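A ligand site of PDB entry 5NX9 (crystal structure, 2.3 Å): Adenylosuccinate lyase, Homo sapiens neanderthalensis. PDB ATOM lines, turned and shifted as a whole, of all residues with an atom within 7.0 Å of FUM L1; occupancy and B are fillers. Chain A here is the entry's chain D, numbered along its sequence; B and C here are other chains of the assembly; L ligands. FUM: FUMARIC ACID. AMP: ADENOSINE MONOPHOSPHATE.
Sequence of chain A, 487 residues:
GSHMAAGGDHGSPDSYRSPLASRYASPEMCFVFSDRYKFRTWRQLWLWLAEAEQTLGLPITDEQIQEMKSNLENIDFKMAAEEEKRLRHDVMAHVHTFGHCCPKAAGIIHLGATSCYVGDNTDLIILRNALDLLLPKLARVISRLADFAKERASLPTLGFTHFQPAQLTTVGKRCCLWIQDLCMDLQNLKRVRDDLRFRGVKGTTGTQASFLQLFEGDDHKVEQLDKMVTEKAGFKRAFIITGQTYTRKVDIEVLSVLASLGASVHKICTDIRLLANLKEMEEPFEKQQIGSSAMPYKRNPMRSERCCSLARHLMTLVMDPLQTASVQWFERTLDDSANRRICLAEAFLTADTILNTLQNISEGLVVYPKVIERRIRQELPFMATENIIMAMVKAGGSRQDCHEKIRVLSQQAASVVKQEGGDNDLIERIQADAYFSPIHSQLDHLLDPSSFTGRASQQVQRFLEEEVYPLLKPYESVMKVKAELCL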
ATOM      1  N   HIS A  89      -8.378  29.521  -9.804  1.00  0.00           N
ATOM      2  CA  HIS A  89      -8.887  28.660 -10.857  1.00  0.00           C
ATOM      3  C   HIS A  89      -7.714  28.012 -11.557  1.00  0.00           C
ATOM      4  O   HIS A  89      -6.975  28.690 -12.263  1.00  0.00           O
ATOM      5  CB  HIS A  89      -9.704  29.476 -11.844  1.00  0.00           C
ATOM      6  CG  HIS A  89     -10.650  28.662 -12.659  1.00  0.00           C
ATOM      7  ND1 HIS A  89     -10.238  27.872 -13.705  1.00  0.00           N
ATOM      8  CD2 HIS A  89     -11.988  28.545 -12.609  1.00  0.00           C
ATOM      9  CE1 HIS A  89     -11.291  27.285 -14.251  1.00  0.00           C
ATOM     10  NE2 HIS A  89     -12.367  27.684 -13.609  1.00  0.00           N
ATOM     11  N   VAL A  91      -7.320  25.843 -14.108  1.00  0.00           N
ATOM     12  CA  VAL A  91      -7.281  25.810 -15.572  1.00  0.00           C
ATOM     13  C   VAL A  91      -6.982  27.179 -16.172  1.00  0.00           C
ATOM     14  O   VAL A  91      -6.183  27.279 -17.098  1.00  0.00           O
ATOM     15  CB  VAL A  91      -8.577  25.201 -16.171  1.00  0.00           C
ATOM     16  CG1 VAL A  91      -8.605  25.325 -17.691  1.00  0.00           C
ATOM     17  CG2 VAL A  91      -8.685  23.733 -15.756  1.00  0.00           C
ATOM     18  N   MET A  92      -7.577  28.230 -15.629  1.00  0.00           N
ATOM     19  CA  MET A  92      -7.368  29.569 -16.178  1.00  0.00           C
ATOM     20  C   MET A  92      -5.941  30.033 -15.878  1.00  0.00           C
ATOM     21  O   MET A  92      -5.333  30.719 -16.689  1.00  0.00           O
ATOM     22  CB  MET A  92      -8.376  30.581 -15.648  1.00  0.00           C
ATOM     23  CG  MET A  92      -9.747  30.475 -16.290  1.00  0.00           C
ATOM     24  SD  MET A  92      -9.849  30.538 -18.084  1.00  0.00           S
ATOM     25  CE  MET A  92      -9.502  32.282 -18.387  1.00  0.00           C
ATOM     26  N   HIS A 110      -7.935  27.378 -25.665  1.00  0.00           N
ATOM     27  CA  HIS A 110      -9.183  27.058 -24.937  1.00  0.00           C
ATOM     28  C   HIS A 110     -10.448  27.567 -25.660  1.00  0.00           C
ATOM     29  O   HIS A 110     -11.514  27.635 -25.060  1.00  0.00           O
ATOM     30  CB  HIS A 110      -9.126  27.642 -23.505  1.00  0.00           C
ATOM     31  CG  HIS A 110      -9.979  26.940 -22.519  1.00  0.00           C
ATOM     32  ND1 HIS A 110      -9.791  25.605 -22.204  1.00  0.00           N
ATOM     33  CD2 HIS A 110     -11.018  27.363 -21.772  1.00  0.00           C
ATOM     34  CE1 HIS A 110     -10.678  25.244 -21.305  1.00  0.00           C
ATOM     35  NE2 HIS A 110     -11.439  26.287 -21.026  1.00  0.00           N
ATOM     36  N   ALA A 113     -14.039  25.929 -25.389  1.00  0.00           N
ATOM     37  CA  ALA A 113     -14.010  24.834 -24.422  1.00  0.00           C
ATOM     38  C   ALA A 113     -14.325  25.274 -22.990  1.00  0.00           C
ATOM     39  O   ALA A 113     -14.164  26.432 -22.636  1.00  0.00           O
ATOM     40  CB  ALA A 113     -12.641  24.164 -24.424  1.00  0.00           C
ATOM     41  N   THR A 114     -14.754  24.327 -22.182  1.00  0.00           N
ATOM     42  CA  THR A 114     -14.863  24.503 -20.742  1.00  0.00           C
ATOM     43  C   THR A 114     -13.657  23.814 -20.091  1.00  0.00           C
ATOM     44  O   THR A 114     -12.942  23.044 -20.743  1.00  0.00           O
ATOM     45  CB  THR A 114     -16.198  23.976 -20.196  1.00  0.00           C
ATOM     46  OG1 THR A 114     -16.366  24.390 -18.825  1.00  0.00           O
ATOM     47  CG2 THR A 114     -16.299  22.445 -20.316  1.00  0.00           C
ATOM     48  N   SER A 115     -13.433  24.097 -18.803  1.00  0.00           N
ATOM     49  CA  SER A 115     -12.260  23.589 -18.101  1.00  0.00           C
ATOM     50  C   SER A 115     -12.076  22.081 -18.202  1.00  0.00           C
ATOM     51  O   SER A 115     -10.965  21.590 -18.329  1.00  0.00           O
ATOM     52  CB  SER A 115     -12.316  23.987 -16.634  1.00  0.00           C
ATOM     53  OG  SER A 115     -12.294  25.388 -16.491  1.00  0.00           O
ATOM     54  N   CYS A 116     -13.188  21.350 -18.129  1.00  0.00           N
ATOM     55  CA  CYS A 116     -13.143  19.882 -18.233  1.00  0.00           C
ATOM     56  C   CYS A 116     -12.634  19.338 -19.555  1.00  0.00           C
ATOM     57  O   CYS A 116     -12.267  18.178 -19.611  1.00  0.00           O
ATOM     58  CB  CYS A 116     -14.517  19.266 -17.965  1.00  0.00           C
ATOM     59  SG  CYS A 116     -14.899  19.240 -16.212  1.00  0.00           S
ATOM     60  N   THR A 204     -19.783  23.739 -21.834  1.00  0.00           N
ATOM     61  CA  THR A 204     -19.990  23.934 -20.395  1.00  0.00           C
ATOM     62  C   THR A 204     -20.999  22.982 -19.747  1.00  0.00           C
ATOM     63  O   THR A 204     -20.810  22.570 -18.608  1.00  0.00           O
ATOM     64  CB  THR A 204     -20.433  25.392 -20.126  1.00  0.00           C
ATOM     65  OG1 THR A 204     -19.435  26.271 -20.625  1.00  0.00           O
ATOM     66  CG2 THR A 204     -20.649  25.649 -18.627  1.00  0.00           C
ATOM     67  N   THR A 205     -22.088  22.663 -20.452  1.00  0.00           N
ATOM     68  CA  THR A 205     -23.150  21.805 -19.906  1.00  0.00           C
ATOM     69  C   THR A 205     -23.396  20.585 -20.772  1.00  0.00           C
ATOM     70  O   THR A 205     -24.388  19.879 -20.567  1.00  0.00           O
ATOM     71  CB  THR A 205     -24.476  22.592 -19.733  1.00  0.00           C
ATOM     72  OG1 THR A 205     -24.858  23.175 -20.978  1.00  0.00           O
ATOM     73  CG2 THR A 205     -24.320  23.699 -18.713  1.00  0.00           C
ATOM     74  N   GLN A 244     -21.280  18.536 -18.052  1.00  0.00           N
ATOM     75  CA  GLN A 244     -19.958  19.144 -18.135  1.00  0.00           C
ATOM     76  C   GLN A 244     -18.847  18.069 -18.104  1.00  0.00           C
ATOM     77  O   GLN A 244     -17.845  18.209 -18.808  1.00  0.00           O
ATOM     78  CB  GLN A 244     -19.747  20.104 -16.999  1.00  0.00           C
ATOM     79  CG  GLN A 244     -18.510  20.943 -17.125  1.00  0.00           C
ATOM     80  CD  GLN A 244     -18.484  22.041 -16.105  1.00  0.00           C
ATOM     81  OE1 GLN A 244     -17.870  21.890 -15.033  1.00  0.00           O
ATOM     82  NE2 GLN A 244     -19.169  23.148 -16.402  1.00  0.00           N
ATOM     83  N   ARG A 332     -23.164  18.792 -13.220  1.00  0.00           N
ATOM     84  CA  ARG A 332     -21.878  18.687 -12.512  1.00  0.00           C
ATOM     85  C   ARG A 332     -21.875  19.522 -11.243  1.00  0.00           C
ATOM     86  O   ARG A 332     -22.318  20.671 -11.288  1.00  0.00           O
ATOM     87  CB  ARG A 332     -20.751  19.229 -13.402  1.00  0.00           C
ATOM     88  CG  ARG A 332     -19.399  18.888 -12.923  1.00  0.00           C
ATOM     89  CD  ARG A 332     -18.726  19.987 -12.146  1.00  0.00           C
ATOM     90  NE  ARG A 332     -17.485  19.371 -11.663  1.00  0.00           N
ATOM     91  CZ  ARG A 332     -16.377  19.334 -12.340  1.00  0.00           C
ATOM     92  NH1 ARG A 332     -16.266  19.982 -13.501  1.00  0.00           N
ATOM     93  NH2 ARG A 332     -15.341  18.696 -11.832  1.00  0.00           N
ATOM     94  N   PHE B 160     -27.305  23.465 -14.921  1.00  0.00           N
ATOM     95  CA  PHE B 160     -26.744  23.709 -13.584  1.00  0.00           C
ATOM     96  C   PHE B 160     -25.398  23.023 -13.430  1.00  0.00           C
ATOM     97  O   PHE B 160     -25.283  21.792 -13.551  1.00  0.00           O
ATOM     98  CB  PHE B 160     -27.685  23.221 -12.471  1.00  0.00           C
ATOM     99  CG  PHE B 160     -28.928  24.040 -12.313  1.00  0.00           C
ATOM    100  CD1 PHE B 160     -28.856  25.339 -11.858  1.00  0.00           C
ATOM    101  CD2 PHE B 160     -30.168  23.498 -12.583  1.00  0.00           C
ATOM    102  CE1 PHE B 160     -30.000  26.102 -11.697  1.00  0.00           C
ATOM    103  CE2 PHE B 160     -31.330  24.245 -12.425  1.00  0.00           C
ATOM    104  CZ  PHE B 160     -31.237  25.559 -11.984  1.00  0.00           C
ATOM    105  N   THR B 161     -24.385  23.835 -13.143  1.00  0.00           N
ATOM    106  CA  THR B 161     -23.091  23.342 -12.703  1.00  0.00           C
ATOM    107  C   THR B 161     -22.786  24.090 -11.423  1.00  0.00           C
ATOM    108  O   THR B 161     -23.099  25.254 -11.305  1.00  0.00           O
ATOM    109  CB  THR B 161     -22.007  23.602 -13.774  1.00  0.00           C
ATOM    110  OG1 THR B 161     -21.885  25.011 -14.025  1.00  0.00           O
ATOM    111  CG2 THR B 161     -22.392  22.926 -15.101  1.00  0.00           C
ATOM    112  N   HIS B 162     -22.204  23.398 -10.454  1.00  0.00           N
ATOM    113  CA  HIS B 162     -22.133  23.873  -9.061  1.00  0.00           C
ATOM    114  C   HIS B 162     -23.521  24.229  -8.507  1.00  0.00           C
ATOM    115  O   HIS B 162     -23.638  25.026  -7.574  1.00  0.00           O
ATOM    116  CB  HIS B 162     -21.235  25.106  -8.914  1.00  0.00           C
ATOM    117  CG  HIS B 162     -19.897  25.015  -9.583  1.00  0.00           C
ATOM    118  ND1 HIS B 162     -18.714  25.056  -8.877  1.00  0.00           N
ATOM    119  CD2 HIS B 162     -19.557  25.027 -10.891  1.00  0.00           C
ATOM    120  CE1 HIS B 162     -17.700  25.046  -9.718  1.00  0.00           C
ATOM    121  NE2 HIS B 162     -18.180  25.035 -10.953  1.00  0.00           N
ATOM    122  N   GLN B 164     -25.408  26.216  -9.934  1.00  0.00           N
ATOM    123  CA  GLN B 164     -25.570  27.610 -10.305  1.00  0.00           C
ATOM    124  C   GLN B 164     -25.957  27.661 -11.773  1.00  0.00           C
ATOM    125  O   GLN B 164     -25.614  26.756 -12.526  1.00  0.00           O
ATOM    126  CB  GLN B 164     -24.258  28.375 -10.086  1.00  0.00           C
ATOM    127  CG  GLN B 164     -23.916  28.586  -8.627  1.00  0.00           C
ATOM    128  CD  GLN B 164     -24.835  29.574  -7.945  1.00  0.00           C
ATOM    129  OE1 GLN B 164     -25.148  30.618  -8.508  1.00  0.00           O
ATOM    130  NE2 GLN B 164     -25.263  29.248  -6.725  1.00  0.00           N
ATOM    131  N   PRO B 165     -26.706  28.700 -12.178  1.00  0.00           N
ATOM    132  CA  PRO B 165     -27.185  28.818 -13.572  1.00  0.00           C
ATOM    133  C   PRO B 165     -26.056  28.704 -14.581  1.00  0.00           C
ATOM    134  O   PRO B 165     -25.013  29.313 -14.403  1.00  0.00           O
ATOM    135  CB  PRO B 165     -27.768  30.216 -13.618  1.00  0.00           C
ATOM    136  CG  PRO B 165     -28.184  30.518 -12.204  1.00  0.00           C
ATOM    137  CD  PRO B 165     -27.215  29.794 -11.322  1.00  0.00           C
ATOM    138  N   ALA B 166     -26.264  27.898 -15.624  1.00  0.00           N
ATOM    139  CA  ALA B 166     -25.261  27.625 -16.643  1.00  0.00           C
ATOM    140  C   ALA B 166     -25.914  27.465 -18.013  1.00  0.00           C
ATOM    141  O   ALA B 166     -27.144  27.410 -18.116  1.00  0.00           O
ATOM    142  CB  ALA B 166     -24.490  26.361 -16.276  1.00  0.00           C
ATOM    143  N   ILE C 290     -12.087  34.046 -10.618  1.00  0.00           N
ATOM    144  CA  ILE C 290     -12.798  33.613 -11.826  1.00  0.00           C
ATOM    145  C   ILE C 290     -13.737  32.455 -11.467  1.00  0.00           C
ATOM    146  O   ILE C 290     -13.360  31.565 -10.689  1.00  0.00           O
ATOM    147  CB  ILE C 290     -11.809  33.211 -12.953  1.00  0.00           C
ATOM    148  CG1 ILE C 290     -11.108  34.444 -13.516  1.00  0.00           C
ATOM    149  CG2 ILE C 290     -12.523  32.487 -14.089  1.00  0.00           C
ATOM    150  CD1 ILE C 290      -9.894  34.121 -14.377  1.00  0.00           C
ATOM    151  N   GLY C 291     -14.947  32.488 -12.017  1.00  0.00           N
ATOM    152  CA  GLY C 291     -15.906  31.399 -11.888  1.00  0.00           C
ATOM    153  C   GLY C 291     -15.755  30.315 -12.937  1.00  0.00           C
ATOM    154  O   GLY C 291     -15.610  29.136 -12.602  1.00  0.00           O
ATOM    155  N   LYS C 298     -20.144  34.470 -12.943  1.00  0.00           N
ATOM    156  CA  LYS C 298     -20.686  33.258 -12.306  1.00  0.00           C
ATOM    157  C   LYS C 298     -20.054  33.014 -10.921  1.00  0.00           C
ATOM    158  O   LYS C 298     -18.836  32.961 -10.791  1.00  0.00           O
ATOM    159  CB  LYS C 298     -20.472  32.024 -13.195  1.00  0.00           C
ATOM    160  CG  LYS C 298     -21.105  30.747 -12.677  1.00  0.00           C
ATOM    161  CD  LYS C 298     -21.359  29.801 -13.838  1.00  0.00           C
ATOM    162  CE  LYS C 298     -22.256  28.636 -13.460  1.00  0.00           C
ATOM    163  NZ  LYS C 298     -21.509  27.520 -12.817  1.00  0.00           N
ATOM    164  N   ASN C 300     -19.564  30.629  -8.043  1.00  0.00           N
ATOM    165  CA  ASN C 300     -19.608  29.229  -7.614  1.00  0.00           C
ATOM    166  C   ASN C 300     -19.181  29.069  -6.158  1.00  0.00           C
ATOM    167  O   ASN C 300     -18.198  29.643  -5.747  1.00  0.00           O
ATOM    168  CB  ASN C 300     -18.722  28.367  -8.520  1.00  0.00           C
ATOM    169  CG  ASN C 300     -19.223  28.306  -9.956  1.00  0.00           C
ATOM    170  OD1 ASN C 300     -20.421  28.324 -10.209  1.00  0.00           O
ATOM    171  ND2 ASN C 300     -18.291  28.213 -10.907  1.00  0.00           N
HETATM  172  OXT FUM L   1     -15.168  25.951 -17.026  1.00  0.00           O
HETATM  173  C   FUM L   1     -15.123  26.474 -15.887  1.00  0.00           C
HETATM  174  O   FUM L   1     -14.078  26.960 -15.432  1.00  0.00           O
HETATM  175  C4  FUM L   1     -16.325  26.578 -15.042  1.00  0.00           C
HETATM  176  C5  FUM L   1     -17.466  25.988 -15.363  1.00  0.00           C
HETATM  177  C6  FUM L   1     -18.644  26.060 -14.447  1.00  0.00           C
HETATM  178  O7  FUM L   1     -18.730  26.936 -13.530  1.00  0.00           O
HETATM  179  O8  FUM L   1     -19.516  25.176 -14.612  1.00  0.00           O
HETATM  180  P   AMP L   2     -10.202  21.591  -5.891  1.00  0.00           P
HETATM  181  O1P AMP L   2     -11.570  21.657  -5.314  1.00  0.00           O
HETATM  182  O2P AMP L   2      -9.937  20.340  -6.712  1.00  0.00           O
HETATM  183  O3P AMP L   2      -9.119  21.954  -4.895  1.00  0.00           O
HETATM  184  O5' AMP L   2     -10.057  22.719  -7.023  1.00  0.00           O
HETATM  185  C5' AMP L   2     -10.939  22.790  -8.139  1.00  0.00           C
HETATM  186  C4' AMP L   2     -10.290  23.718  -9.149  1.00  0.00           C
HETATM  187  O4' AMP L   2     -11.064  23.731 -10.360  1.00  0.00           O
HETATM  188  C3' AMP L   2     -10.229  25.138  -8.607  1.00  0.00           C
HETATM  189  O3' AMP L   2      -9.061  25.840  -9.021  1.00  0.00           O
HETATM  190  C2' AMP L   2     -11.454  25.751  -9.223  1.00  0.00           C
HETATM  191  O2' AMP L   2     -11.429  27.184  -9.263  1.00  0.00           O
HETATM  192  C1' AMP L   2     -11.479  25.082 -10.604  1.00  0.00           C
HETATM  193  N9  AMP L   2     -12.825  25.072 -11.164  1.00  0.00           N
HETATM  194  C8  AMP L   2     -13.862  25.864 -10.804  1.00  0.00           C
HETATM  195  N7  AMP L   2     -14.969  25.528 -11.512  1.00  0.00           N
HETATM  196  C5  AMP L   2     -14.618  24.524 -12.324  1.00  0.00           C
HETATM  197  C6  AMP L   2     -15.298  23.713 -13.333  1.00  0.00           C
HETATM  198  N6  AMP L   2     -16.585  23.940 -13.577  1.00  0.00           N
HETATM  199  N1  AMP L   2     -14.616  22.760 -13.953  1.00  0.00           N
HETATM  200  C2  AMP L   2     -13.332  22.526 -13.685  1.00  0.00           C
HETATM  201  N3  AMP L   2     -12.648  23.233 -12.788  1.00  0.00           N
HETATM  202  C4  AMP L   2     -13.233  24.212 -12.081  1.00  0.00           C
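The side-chain amino group (NZ) of Lys 298 of chain C lies within salt-bridge range of an oxygen (O7) of FUM L1. The side-chain hydroxyl (OG) of Ser 115 sits at hydrogen-bond distance from an oxygen (O) of FUM L1 (2.6 Å). A ring nitrogen (NE2) of His 162 of chain B sits at hydrogen-bond distance from an oxygen (O7) of FUM L1 (3.2 Å). An oxygen (OXT) of FUM L1 lies within hydrogen-bond range of the backbone NH (N) of Ser 115, 3.1 Å away. NE2 of His 162 of chain B sits at hydrogen-bond distance from N6 of AMP L2, at 3.3 Å. The side-chain amide nitrogen (NE2) of Gln 244 is in hydrogen-bond range of an oxygen (O8) of FUM L1 (2.7 Å). OE1 of Gln 244 lies within hydrogen-bond range of N6 of AMP L2, 2.8 Å away. The side-chain hydroxyl (OG1) of Thr 114 sits at hydrogen-bond distance from an oxygen (OXT) of FUM L1, 2.7 Å away. OG1 of Thr 161 of chain B is in hydrogen-bond range of O8 of FUM L1 (2.4 Å). The side-chain amide nitrogen (ND2) of Asn 300 of chain C is in hydrogen-bond range of an oxygen (O7) of FUM L1 (3.0 Å). An oxygen (O) of FUM L1 lies within hydrogen-bond range of a ring nitrogen (NE2) of His 89, 2.6 Å away. NH1 of Arg 332 sits at hydrogen-bond distance from N1 of AMP L2.
An oxygen (O8) of FUM L1 sits close to a nitrogen (N6) of AMP L2.
The guanidinium group (NH1) of Arg 332 sits at hydrogen-bond distance from the side-chain amide oxygen (OE1) of Gln 244, 2.9 Å away. The side-chain amino group (NZ) of Lys 298 of chain C is in hydrogen-bond range of the side-chain amide oxygen (OD1) of Asn 300 of chain C (2.9 Å). A ring nitrogen (ND1) of His 89 is in hydrogen-bond range of the backbone NH (N) of Met 92. N of His 162 of chain B sits at hydrogen-bond distance from O of Arg 332, 2.9 Å away. The side-chain hydroxyl (OG1) of Thr 161 of chain B lies within hydrogen-bond range of the side-chain amino group (NZ) of Lys 298 of chain C (2.8 Å). The side-chain amide nitrogen of Asn 300 of chain C sits at hydrogen-bond distance from the backbone carbonyl oxygen of Gly 291 of chain C (3.3 Å). ND2 of Asn 300 of chain C lies within hydrogen-bond range of NE2 of His 162 of chain B (3.2 Å). NE2 of Gln 244 sits at hydrogen-bond distance from O of Thr 204 (2.8 Å).
Merely in contact with FUM L1: Gly 291 of chain C (3.6 Å). Hydrophobic or aromatic side chains within 4 Å of FUM L1: His 89 and His 162 of chain B. The nearest printed residue that does not touch FUM L1 is Thr 204 (4.2 Å).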
